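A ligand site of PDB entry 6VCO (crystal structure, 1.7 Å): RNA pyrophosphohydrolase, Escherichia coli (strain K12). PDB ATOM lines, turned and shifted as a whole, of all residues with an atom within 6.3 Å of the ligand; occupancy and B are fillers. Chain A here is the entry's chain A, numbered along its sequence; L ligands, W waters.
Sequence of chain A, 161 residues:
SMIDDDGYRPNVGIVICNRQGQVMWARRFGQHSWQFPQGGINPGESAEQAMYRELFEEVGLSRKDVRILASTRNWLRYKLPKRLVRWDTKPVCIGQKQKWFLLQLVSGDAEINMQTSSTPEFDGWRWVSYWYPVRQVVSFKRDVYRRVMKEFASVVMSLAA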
ATOM      1  N   ARG A   9     -18.272 -20.191 -15.008  1.00  0.00           N
ATOM      2  CA  ARG A   9     -18.462 -21.564 -15.446  1.00  0.00           C
ATOM      3  C   ARG A   9     -19.759 -22.095 -14.844  1.00  0.00           C
ATOM      4  O   ARG A   9     -19.966 -21.896 -13.638  1.00  0.00           O
ATOM      5  CB  ARG A   9     -17.311 -22.468 -15.023  1.00  0.00           C
ATOM      6  CG  ARG A   9     -16.093 -22.392 -15.947  1.00  0.00           C
ATOM      7  CD  ARG A   9     -14.982 -23.382 -15.557  1.00  0.00           C
ATOM      8  NE  ARG A   9     -14.891 -23.481 -14.114  1.00  0.00           N
ATOM      9  CZ  ARG A   9     -13.766 -23.309 -13.404  1.00  0.00           C
ATOM     10  NH1 ARG A   9     -12.614 -23.033 -14.015  1.00  0.00           N
ATOM     11  NH2 ARG A   9     -13.814 -23.404 -12.076  1.00  0.00           N
ATOM     12  N   ASN A  11     -22.106 -24.661 -13.070  1.00  0.00           N
ATOM     13  CA  ASN A  11     -21.864 -25.759 -12.138  1.00  0.00           C
ATOM     14  C   ASN A  11     -23.174 -26.159 -11.461  1.00  0.00           C
ATOM     15  O   ASN A  11     -24.166 -25.434 -11.516  1.00  0.00           O
ATOM     16  CB  ASN A  11     -20.787 -25.355 -11.115  1.00  0.00           C
ATOM     17  CG  ASN A  11     -19.373 -25.455 -11.687  1.00  0.00           C
ATOM     18  OD1 ASN A  11     -18.704 -26.441 -11.497  1.00  0.00           O
ATOM     19  ND2 ASN A  11     -18.931 -24.417 -12.402  1.00  0.00           N
ATOM     20  N   ARG A  28     -12.834 -31.012   1.825  1.00  0.00           N
ATOM     21  CA  ARG A  28     -12.115 -30.860   0.559  1.00  0.00           C
ATOM     22  C   ARG A  28     -10.811 -31.645   0.611  1.00  0.00           C
ATOM     23  O   ARG A  28     -10.093 -31.599   1.617  1.00  0.00           O
ATOM     24  CB  ARG A  28     -11.821 -29.379   0.244  1.00  0.00           C
ATOM     25  CG  ARG A  28     -13.081 -28.574  -0.125  1.00  0.00           C
ATOM     26  CD  ARG A  28     -12.752 -27.089  -0.412  1.00  0.00           C
ATOM     27  NE  ARG A  28     -11.731 -26.954  -1.471  1.00  0.00           N
ATOM     28  CZ  ARG A  28     -11.995 -26.769  -2.766  1.00  0.00           C
ATOM     29  NH1 ARG A  28     -10.999 -26.694  -3.646  1.00  0.00           N
ATOM     30  NH2 ARG A  28     -13.233 -26.697  -3.188  1.00  0.00           N
ATOM     31  N   GLN A  31      -7.413 -30.836   2.613  1.00  0.00           N
ATOM     32  CA  GLN A  31      -7.647 -29.543   3.242  1.00  0.00           C
ATOM     33  C   GLN A  31      -8.376 -29.755   4.571  1.00  0.00           C
ATOM     34  O   GLN A  31      -8.768 -30.864   4.918  1.00  0.00           O
ATOM     35  CB  GLN A  31      -8.479 -28.634   2.351  1.00  0.00           C
ATOM     36  CG  GLN A  31      -7.835 -28.339   1.022  1.00  0.00           C
ATOM     37  CD  GLN A  31      -6.580 -27.559   1.190  1.00  0.00           C
ATOM     38  OE1 GLN A  31      -6.551 -26.550   1.906  1.00  0.00           O
ATOM     39  NE2 GLN A  31      -5.525 -27.998   0.533  1.00  0.00           N
ATOM     40  N   SER A  33     -10.938 -27.519   5.052  1.00  0.00           N
ATOM     41  CA  SER A  33     -12.110 -26.767   4.648  1.00  0.00           C
ATOM     42  C   SER A  33     -13.140 -27.731   4.086  1.00  0.00           C
ATOM     43  O   SER A  33     -12.781 -28.740   3.473  1.00  0.00           O
ATOM     44  CB  SER A  33     -11.743 -25.742   3.562  1.00  0.00           C
ATOM     45  OG  SER A  33     -10.979 -26.355   2.562  1.00  0.00           O
ATOM     46  N   TRP A  34     -14.409 -27.431   4.331  1.00  0.00           N
ATOM     47  CA  TRP A  34     -15.483 -28.346   4.026  1.00  0.00           C
ATOM     48  C   TRP A  34     -16.519 -27.648   3.149  1.00  0.00           C
ATOM     49  O   TRP A  34     -16.614 -26.412   3.118  1.00  0.00           O
ATOM     50  CB  TRP A  34     -16.138 -28.813   5.293  1.00  0.00           C
ATOM     51  CG  TRP A  34     -15.273 -29.618   6.207  1.00  0.00           C
ATOM     52  CD1 TRP A  34     -14.137 -29.215   6.843  1.00  0.00           C
ATOM     53  CD2 TRP A  34     -15.503 -30.981   6.618  1.00  0.00           C
ATOM     54  NE1 TRP A  34     -13.635 -30.238   7.635  1.00  0.00           N
ATOM     55  CE2 TRP A  34     -14.457 -31.326   7.513  1.00  0.00           C
ATOM     56  CE3 TRP A  34     -16.488 -31.927   6.331  1.00  0.00           C
ATOM     57  CZ2 TRP A  34     -14.353 -32.594   8.078  1.00  0.00           C
ATOM     58  CZ3 TRP A  34     -16.401 -33.176   6.935  1.00  0.00           C
ATOM     59  CH2 TRP A  34     -15.341 -33.479   7.821  1.00  0.00           C
ATOM     60  N   GLN A  35     -17.293 -28.439   2.432  1.00  0.00           N
ATOM     61  CA  GLN A  35     -18.265 -27.916   1.493  1.00  0.00           C
ATOM     62  C   GLN A  35     -19.223 -29.023   1.061  1.00  0.00           C
ATOM     63  O   GLN A  35     -19.048 -30.207   1.382  1.00  0.00           O
ATOM     64  CB  GLN A  35     -17.592 -27.286   0.274  1.00  0.00           C
ATOM     65  CG  GLN A  35     -17.025 -28.310  -0.714  1.00  0.00           C
ATOM     66  CD  GLN A  35     -16.413 -27.686  -1.972  1.00  0.00           C
ATOM     67  OE1 GLN A  35     -15.873 -26.577  -1.913  1.00  0.00           O
ATOM     68  NE2 GLN A  35     -16.455 -28.411  -3.081  1.00  0.00           N
ATOM     69  N   GLN A  38     -19.946 -30.130  -5.503  1.00  0.00           N
ATOM     70  CA  GLN A  38     -20.248 -29.273  -6.646  1.00  0.00           C
ATOM     71  C   GLN A  38     -19.423 -29.672  -7.861  1.00  0.00           C
ATOM     72  O   GLN A  38     -18.285 -30.100  -7.712  1.00  0.00           O
ATOM     73  CB  GLN A  38     -20.050 -27.801  -6.316  1.00  0.00           C
ATOM     74  CG  GLN A  38     -18.689 -27.399  -5.889  1.00  0.00           C
ATOM     75  CD  GLN A  38     -18.568 -25.908  -5.778  1.00  0.00           C
ATOM     76  OE1 GLN A  38     -19.001 -25.322  -4.780  1.00  0.00           O
ATOM     77  NE2 GLN A  38     -17.993 -25.284  -6.801  1.00  0.00           N
ATOM     78  N   GLY A  39     -20.034 -29.590  -9.041  1.00  0.00           N
ATOM     79  CA  GLY A  39     -19.374 -30.106 -10.231  1.00  0.00           C
ATOM     80  C   GLY A  39     -19.790 -29.332 -11.450  1.00  0.00           C
ATOM     81  O   GLY A  39     -20.815 -28.649 -11.466  1.00  0.00           O
ATOM     82  N   GLY A  40     -18.947 -29.415 -12.461  1.00  0.00           N
ATOM     83  CA  GLY A  40     -19.232 -28.698 -13.691  1.00  0.00           C
ATOM     84  C   GLY A  40     -20.254 -29.346 -14.593  1.00  0.00           C
ATOM     85  O   GLY A  40     -20.654 -30.508 -14.447  1.00  0.00           O
ATOM     86  N   TYR A  78     -21.211 -16.901  -7.607  1.00  0.00           N
ATOM     87  CA  TYR A  78     -20.190 -16.374  -6.709  1.00  0.00           C
ATOM     88  C   TYR A  78     -18.951 -16.022  -7.505  1.00  0.00           C
ATOM     89  O   TYR A  78     -18.658 -16.623  -8.550  1.00  0.00           O
ATOM     90  CB  TYR A  78     -19.822 -17.315  -5.536  1.00  0.00           C
ATOM     91  CG  TYR A  78     -19.145 -18.629  -5.865  1.00  0.00           C
ATOM     92  CD1 TYR A  78     -17.811 -18.704  -6.240  1.00  0.00           C
ATOM     93  CD2 TYR A  78     -19.845 -19.823  -5.761  1.00  0.00           C
ATOM     94  CE1 TYR A  78     -17.208 -19.925  -6.521  1.00  0.00           C
ATOM     95  CE2 TYR A  78     -19.261 -21.045  -6.033  1.00  0.00           C
ATOM     96  CZ  TYR A  78     -17.951 -21.103  -6.409  1.00  0.00           C
ATOM     97  OH  TYR A  78     -17.364 -22.315  -6.673  1.00  0.00           O
ATOM     98  N   LEU A  80     -14.820 -15.454  -7.561  1.00  0.00           N
ATOM     99  CA  LEU A  80     -13.614 -15.907  -6.894  1.00  0.00           C
ATOM    100  C   LEU A  80     -12.869 -14.719  -6.307  1.00  0.00           C
ATOM    101  O   LEU A  80     -12.825 -13.649  -6.926  1.00  0.00           O
ATOM    102  CB  LEU A  80     -12.695 -16.636  -7.868  1.00  0.00           C
ATOM    103  CG  LEU A  80     -13.124 -18.022  -8.353  1.00  0.00           C
ATOM    104  CD1 LEU A  80     -12.196 -18.470  -9.446  1.00  0.00           C
ATOM    105  CD2 LEU A  80     -13.124 -18.969  -7.192  1.00  0.00           C
ATOM    106  N   PRO A  81     -12.256 -14.872  -5.135  1.00  0.00           N
ATOM    107  CA  PRO A  81     -11.268 -13.883  -4.687  1.00  0.00           C
ATOM    108  C   PRO A  81     -10.237 -13.657  -5.777  1.00  0.00           C
ATOM    109  O   PRO A  81      -9.793 -14.588  -6.454  1.00  0.00           O
ATOM    110  CB  PRO A  81     -10.649 -14.536  -3.455  1.00  0.00           C
ATOM    111  CG  PRO A  81     -11.750 -15.421  -2.929  1.00  0.00           C
ATOM    112  CD  PRO A  81     -12.470 -15.943  -4.135  1.00  0.00           C
ATOM    113  N   LEU A  84      -7.308 -15.867  -6.268  1.00  0.00           N
ATOM    114  CA  LEU A  84      -7.479 -17.257  -6.669  1.00  0.00           C
ATOM    115  C   LEU A  84      -7.822 -17.424  -8.139  1.00  0.00           C
ATOM    116  O   LEU A  84      -8.062 -18.550  -8.590  1.00  0.00           O
ATOM    117  CB  LEU A  84      -8.573 -17.925  -5.809  1.00  0.00           C
ATOM    118  CG  LEU A  84      -8.330 -17.948  -4.307  1.00  0.00           C
ATOM    119  CD1 LEU A  84      -9.520 -18.546  -3.551  1.00  0.00           C
ATOM    120  CD2 LEU A  84      -7.034 -18.699  -3.968  1.00  0.00           C
ATOM    121  N   GLN A  96     -18.441 -18.814 -10.639  1.00  0.00           N
ATOM    122  CA  GLN A  96     -19.313 -19.902 -11.045  1.00  0.00           C
ATOM    123  C   GLN A  96     -20.758 -19.411 -11.007  1.00  0.00           C
ATOM    124  O   GLN A  96     -21.126 -18.600 -10.160  1.00  0.00           O
ATOM    125  CB  GLN A  96     -19.160 -21.139 -10.142  1.00  0.00           C
ATOM    126  CG  GLN A  96     -17.809 -21.831 -10.236  1.00  0.00           C
ATOM    127  CD  GLN A  96     -17.827 -23.231  -9.653  1.00  0.00           C
ATOM    128  OE1 GLN A  96     -18.885 -23.752  -9.300  1.00  0.00           O
ATOM    129  NE2 GLN A  96     -16.654 -23.847  -9.564  1.00  0.00           N
ATOM    130  N   GLN A 136     -19.898 -22.226   8.178  1.00  0.00           N
ATOM    131  CA  GLN A 136     -18.627 -22.926   8.076  1.00  0.00           C
ATOM    132  C   GLN A 136     -18.014 -22.917   6.690  1.00  0.00           C
ATOM    133  O   GLN A 136     -16.822 -23.223   6.567  1.00  0.00           O
ATOM    134  CB  GLN A 136     -18.808 -24.385   8.526  1.00  0.00           C
ATOM    135  CG  GLN A 136     -19.123 -24.524   9.986  1.00  0.00           C
ATOM    136  CD  GLN A 136     -17.894 -24.409  10.872  1.00  0.00           C
ATOM    137  OE1 GLN A 136     -17.940 -23.814  11.951  1.00  0.00           O
ATOM    138  NE2 GLN A 136     -16.790 -24.980  10.420  1.00  0.00           N
ATOM    139  N   VAL A 137     -18.771 -22.606   5.648  1.00  0.00           N
ATOM    140  CA  VAL A 137     -18.194 -22.580   4.310  1.00  0.00           C
ATOM    141  C   VAL A 137     -17.326 -21.330   4.150  1.00  0.00           C
ATOM    142  O   VAL A 137     -17.520 -20.315   4.810  1.00  0.00           O
ATOM    143  CB  VAL A 137     -19.294 -22.645   3.233  1.00  0.00           C
ATOM    144  CG1 VAL A 137     -20.069 -21.326   3.146  1.00  0.00           C
ATOM    145  CG2 VAL A 137     -18.682 -22.997   1.869  1.00  0.00           C
ATOM    146  N   VAL A 138     -16.351 -21.429   3.234  1.00  0.00           N
ATOM    147  CA  VAL A 138     -15.469 -20.301   2.933  1.00  0.00           C
ATOM    148  C   VAL A 138     -16.306 -19.062   2.616  1.00  0.00           C
ATOM    149  O   VAL A 138     -17.361 -19.146   1.980  1.00  0.00           O
ATOM    150  CB  VAL A 138     -14.550 -20.661   1.762  1.00  0.00           C
ATOM    151  CG1 VAL A 138     -15.330 -20.768   0.459  1.00  0.00           C
ATOM    152  CG2 VAL A 138     -13.411 -19.656   1.618  1.00  0.00           C
ATOM    153  N   PHE A 140     -16.310 -16.541   0.587  1.00  0.00           N
ATOM    154  CA  PHE A 140     -16.783 -16.106  -0.730  1.00  0.00           C
ATOM    155  C   PHE A 140     -17.962 -16.934  -1.256  1.00  0.00           C
ATOM    156  O   PHE A 140     -18.614 -16.501  -2.209  1.00  0.00           O
ATOM    157  CB  PHE A 140     -15.640 -16.019  -1.773  1.00  0.00           C
ATOM    158  CG  PHE A 140     -15.030 -17.342  -2.205  1.00  0.00           C
ATOM    159  CD1 PHE A 140     -15.545 -18.033  -3.283  1.00  0.00           C
ATOM    160  CD2 PHE A 140     -13.886 -17.822  -1.585  1.00  0.00           C
ATOM    161  CE1 PHE A 140     -14.957 -19.217  -3.712  1.00  0.00           C
ATOM    162  CE2 PHE A 140     -13.285 -19.006  -2.010  1.00  0.00           C
ATOM    163  CZ  PHE A 140     -13.828 -19.699  -3.076  1.00  0.00           C
ATOM    164  N   LYS A 141     -18.293 -18.063  -0.628  1.00  0.00           N
ATOM    165  CA  LYS A 141     -19.473 -18.818  -1.017  1.00  0.00           C
ATOM    166  C   LYS A 141     -20.641 -18.648  -0.053  1.00  0.00           C
ATOM    167  O   LYS A 141     -21.731 -19.202  -0.296  1.00  0.00           O
ATOM    168  CB  LYS A 141     -19.147 -20.316  -1.137  1.00  0.00           C
ATOM    169  CG  LYS A 141     -18.088 -20.638  -2.131  1.00  0.00           C
ATOM    170  CD  LYS A 141     -17.879 -22.166  -2.199  1.00  0.00           C
ATOM    171  CE  LYS A 141     -16.787 -22.496  -3.196  1.00  0.00           C
ATOM    172  NZ  LYS A 141     -16.709 -23.929  -3.463  1.00  0.00           N
HETATM  173  P1  LIG L   1     -12.852 -27.428 -10.030  1.00  0.00           P
HETATM  174  O1  LIG L   1     -14.182 -28.136 -10.279  1.00  0.00           O
HETATM  175  O2  LIG L   1     -12.927 -25.995 -10.519  1.00  0.00           O
HETATM  176  O3  LIG L   1     -11.655 -28.134 -10.745  1.00  0.00           O
HETATM  177  P2  LIG L   1     -12.361 -26.134  -7.478  1.00  0.00           P
HETATM  178  O4  LIG L   1     -12.379 -26.626  -6.040  1.00  0.00           O
HETATM  179  O5  LIG L   1     -11.006 -25.421  -7.766  1.00  0.00           O
HETATM  180  O6  LIG L   1     -12.580 -27.357  -8.469  1.00  0.00           O
HETATM  181  P3  LIG L   1     -14.074 -23.745  -6.438  1.00  0.00           P
HETATM  182  O7  LIG L   1     -14.814 -22.560  -6.992  1.00  0.00           O
HETATM  183  O8  LIG L   1     -14.780 -24.470  -5.264  1.00  0.00           O
HETATM  184  C1  LIG L   1     -13.763 -24.901  -7.831  1.00  0.00           C
HETATM  185  O9  LIG L   1     -12.661 -23.275  -5.906  1.00  0.00           O
HETATM  186  C2  LIG L   1     -11.838 -22.311  -6.697  1.00  0.00           C
HETATM  187  C3  LIG L   1     -10.578 -22.104  -5.896  1.00  0.00           C
HETATM  188  O10 LIG L   1     -11.021 -21.596  -4.615  1.00  0.00           O
HETATM  189  C4  LIG L   1      -9.890 -23.378  -5.576  1.00  0.00           C
HETATM  190  O11 LIG L   1      -8.638 -23.516  -6.272  1.00  0.00           O
HETATM  191  C5  LIG L   1      -9.702 -23.265  -4.046  1.00  0.00           C
HETATM  192  O12 LIG L   1      -8.314 -23.264  -3.716  1.00  0.00           O
HETATM  193  C6  LIG L   1     -10.256 -22.167  -3.583  1.00  0.00           C
HETATM  194  N1  LIG L   1     -11.102 -22.555  -2.455  1.00  0.00           N
HETATM  195  C7  LIG L   1     -12.337 -23.131  -2.534  1.00  0.00           C
HETATM  196  N2  LIG L   1     -12.888 -23.398  -1.335  1.00  0.00           N
HETATM  197  C8  LIG L   1     -11.909 -22.936  -0.447  1.00  0.00           C
HETATM  198  C9  LIG L   1     -11.860 -22.940   0.943  1.00  0.00           C
HETATM  199  N3  LIG L   1     -12.884 -23.401   1.683  1.00  0.00           N
HETATM  200  N4  LIG L   1     -10.863 -22.459   1.581  1.00  0.00           N
HETATM  201  C10 LIG L   1      -9.845 -21.978   0.831  1.00  0.00           C
HETATM  202  N5  LIG L   1      -9.772 -21.931  -0.473  1.00  0.00           N
HETATM  203  C11 LIG L   1     -10.834 -22.418  -1.158  1.00  0.00           C
HETATM  204  O   HOH W   1     -15.325 -24.294  -0.801  1.00  0.00           O
HETATM  205  O   HOH W   2     -14.140 -21.659  -9.585  1.00  0.00           O
HETATM  206  O   HOH W   3     -15.504 -27.176  -5.377  1.00  0.00           O
HETATM  207  O   HOH W   4      -8.603 -24.786   2.376  1.00  0.00           O
HETATM  208  O   HOH W   5     -16.062 -26.993 -12.068  1.00  0.00           O
HETATM  209  O   HOH W   6     -16.980 -26.986  -8.973  1.00  0.00           O
HETATM  210  O   HOH W   7     -12.707 -29.399  -5.820  1.00  0.00           O
HETATM  211  O   HOH W   8     -12.861 -22.694   4.421  1.00  0.00           O
HETATM  212  O   HOH W   9     -15.434 -24.271   2.090  1.00  0.00           O
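The side-chain hydroxyl (OH) of Tyr 78 lies within hydrogen-bond range of the side-chain amide nitrogen (NE2) of Gln 38 (3.0 Å). NZ of Lys 141 is in hydrogen-bond range of OE1 of Gln 38. The side-chain amide oxygen (OE1) of Gln 35 sits at hydrogen-bond distance from the side-chain amino group (NZ) of Lys 141 (3.2 Å). The backbone NH (N) of Arg 28 sits at hydrogen-bond distance from the backbone carbonyl oxygen (O) of Ser 33 (2.8 Å). NH2 of Arg 28 is in hydrogen-bond range of OE1 of Gln 35, 2.9 Å away. The backbone carbonyl oxygen (O) of Arg 9 is in hydrogen-bond range of the side-chain amide nitrogen (ND2) of Asn 11 (3.0 Å). The side-chain amide nitrogen (NE2) of Gln 38 lies within hydrogen-bond range of the side-chain amide oxygen (OE1) of Gln 96, 3.1 Å away. ND2 of Asn 11 sits close to OE1 of Gln 96 (3.2 Å).
Ser 33 touches the ligand (CB to N3, 3.2 Å). Gln 38 touches the ligand. Leu 80 touches the ligand (CD2 to C2, 3.6 Å). Leu 84 touches the ligand. CB of Val 138 touches N3 of the ligand, at 3.2 Å. Phe 140 touches the ligand (CZ to O10, 3.7 Å). Hydrophobic or aromatic side chains that line the ligand: Tyr 78, Leu 80, Leu 84, Val 138 and Phe 140. 11 residues have an atom within 4 Å of the ligand: Arg 9, Arg 28, Ser 33, Gln 38, Tyr 78, Leu 80, Leu 84, Gln 96, Val 138, Phe 140 and Lys 141.
Water W1 lies within hydrogen-bond range of the side-chain amide oxygen (OE1) of Gln 35 (2.6 Å), a nitrogen (N2) of the ligand (2.7 Å) and the side-chain amino group (NZ) of Lys 141 (3.0 Å). Water W9 lies within hydrogen-bond range of O of Trp 34, N3 of the ligand and N of Val 138. Water W2 lies within hydrogen-bond range of O7 of the ligand, NH2 of Arg 9 and NE2 of Gln 96. Water W5 lies within hydrogen-bond range of the side-chain amide oxygen (OD1) of Asn 11 and an oxygen (O1) of the ligand. Water W6 lies within hydrogen-bond range of the side-chain amide nitrogen of Gln 38, the side-chain amide oxygen of Asn 11, the side-chain amide nitrogen of Gln 96 and an oxygen (O1) of the ligand. Water W4 lies within hydrogen-bond range of OE1 of Gln 31 (2.7 Å), OG of Ser 33 (2.9 Å) and N4 of the ligand (3.3 Å).
O7 of the ligand lies within hydrogen-bond range of OH of Tyr 78 (2.6 Å). NZ of Lys 141 is in salt-bridge range of O8 of the ligand, 2.7 Å away. The guanidinium group (NH1) of Arg 28 is in salt-bridge range of an oxygen (O4) of the ligand. An oxygen (O2) of the ligand is in salt-bridge range of the guanidinium group (NH2) of Arg 9, at 3.2 Å. An oxygen (O7) of the ligand sits at hydrogen-bond distance from the side-chain amide nitrogen (NE2) of Gln 96 (3.4 Å).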
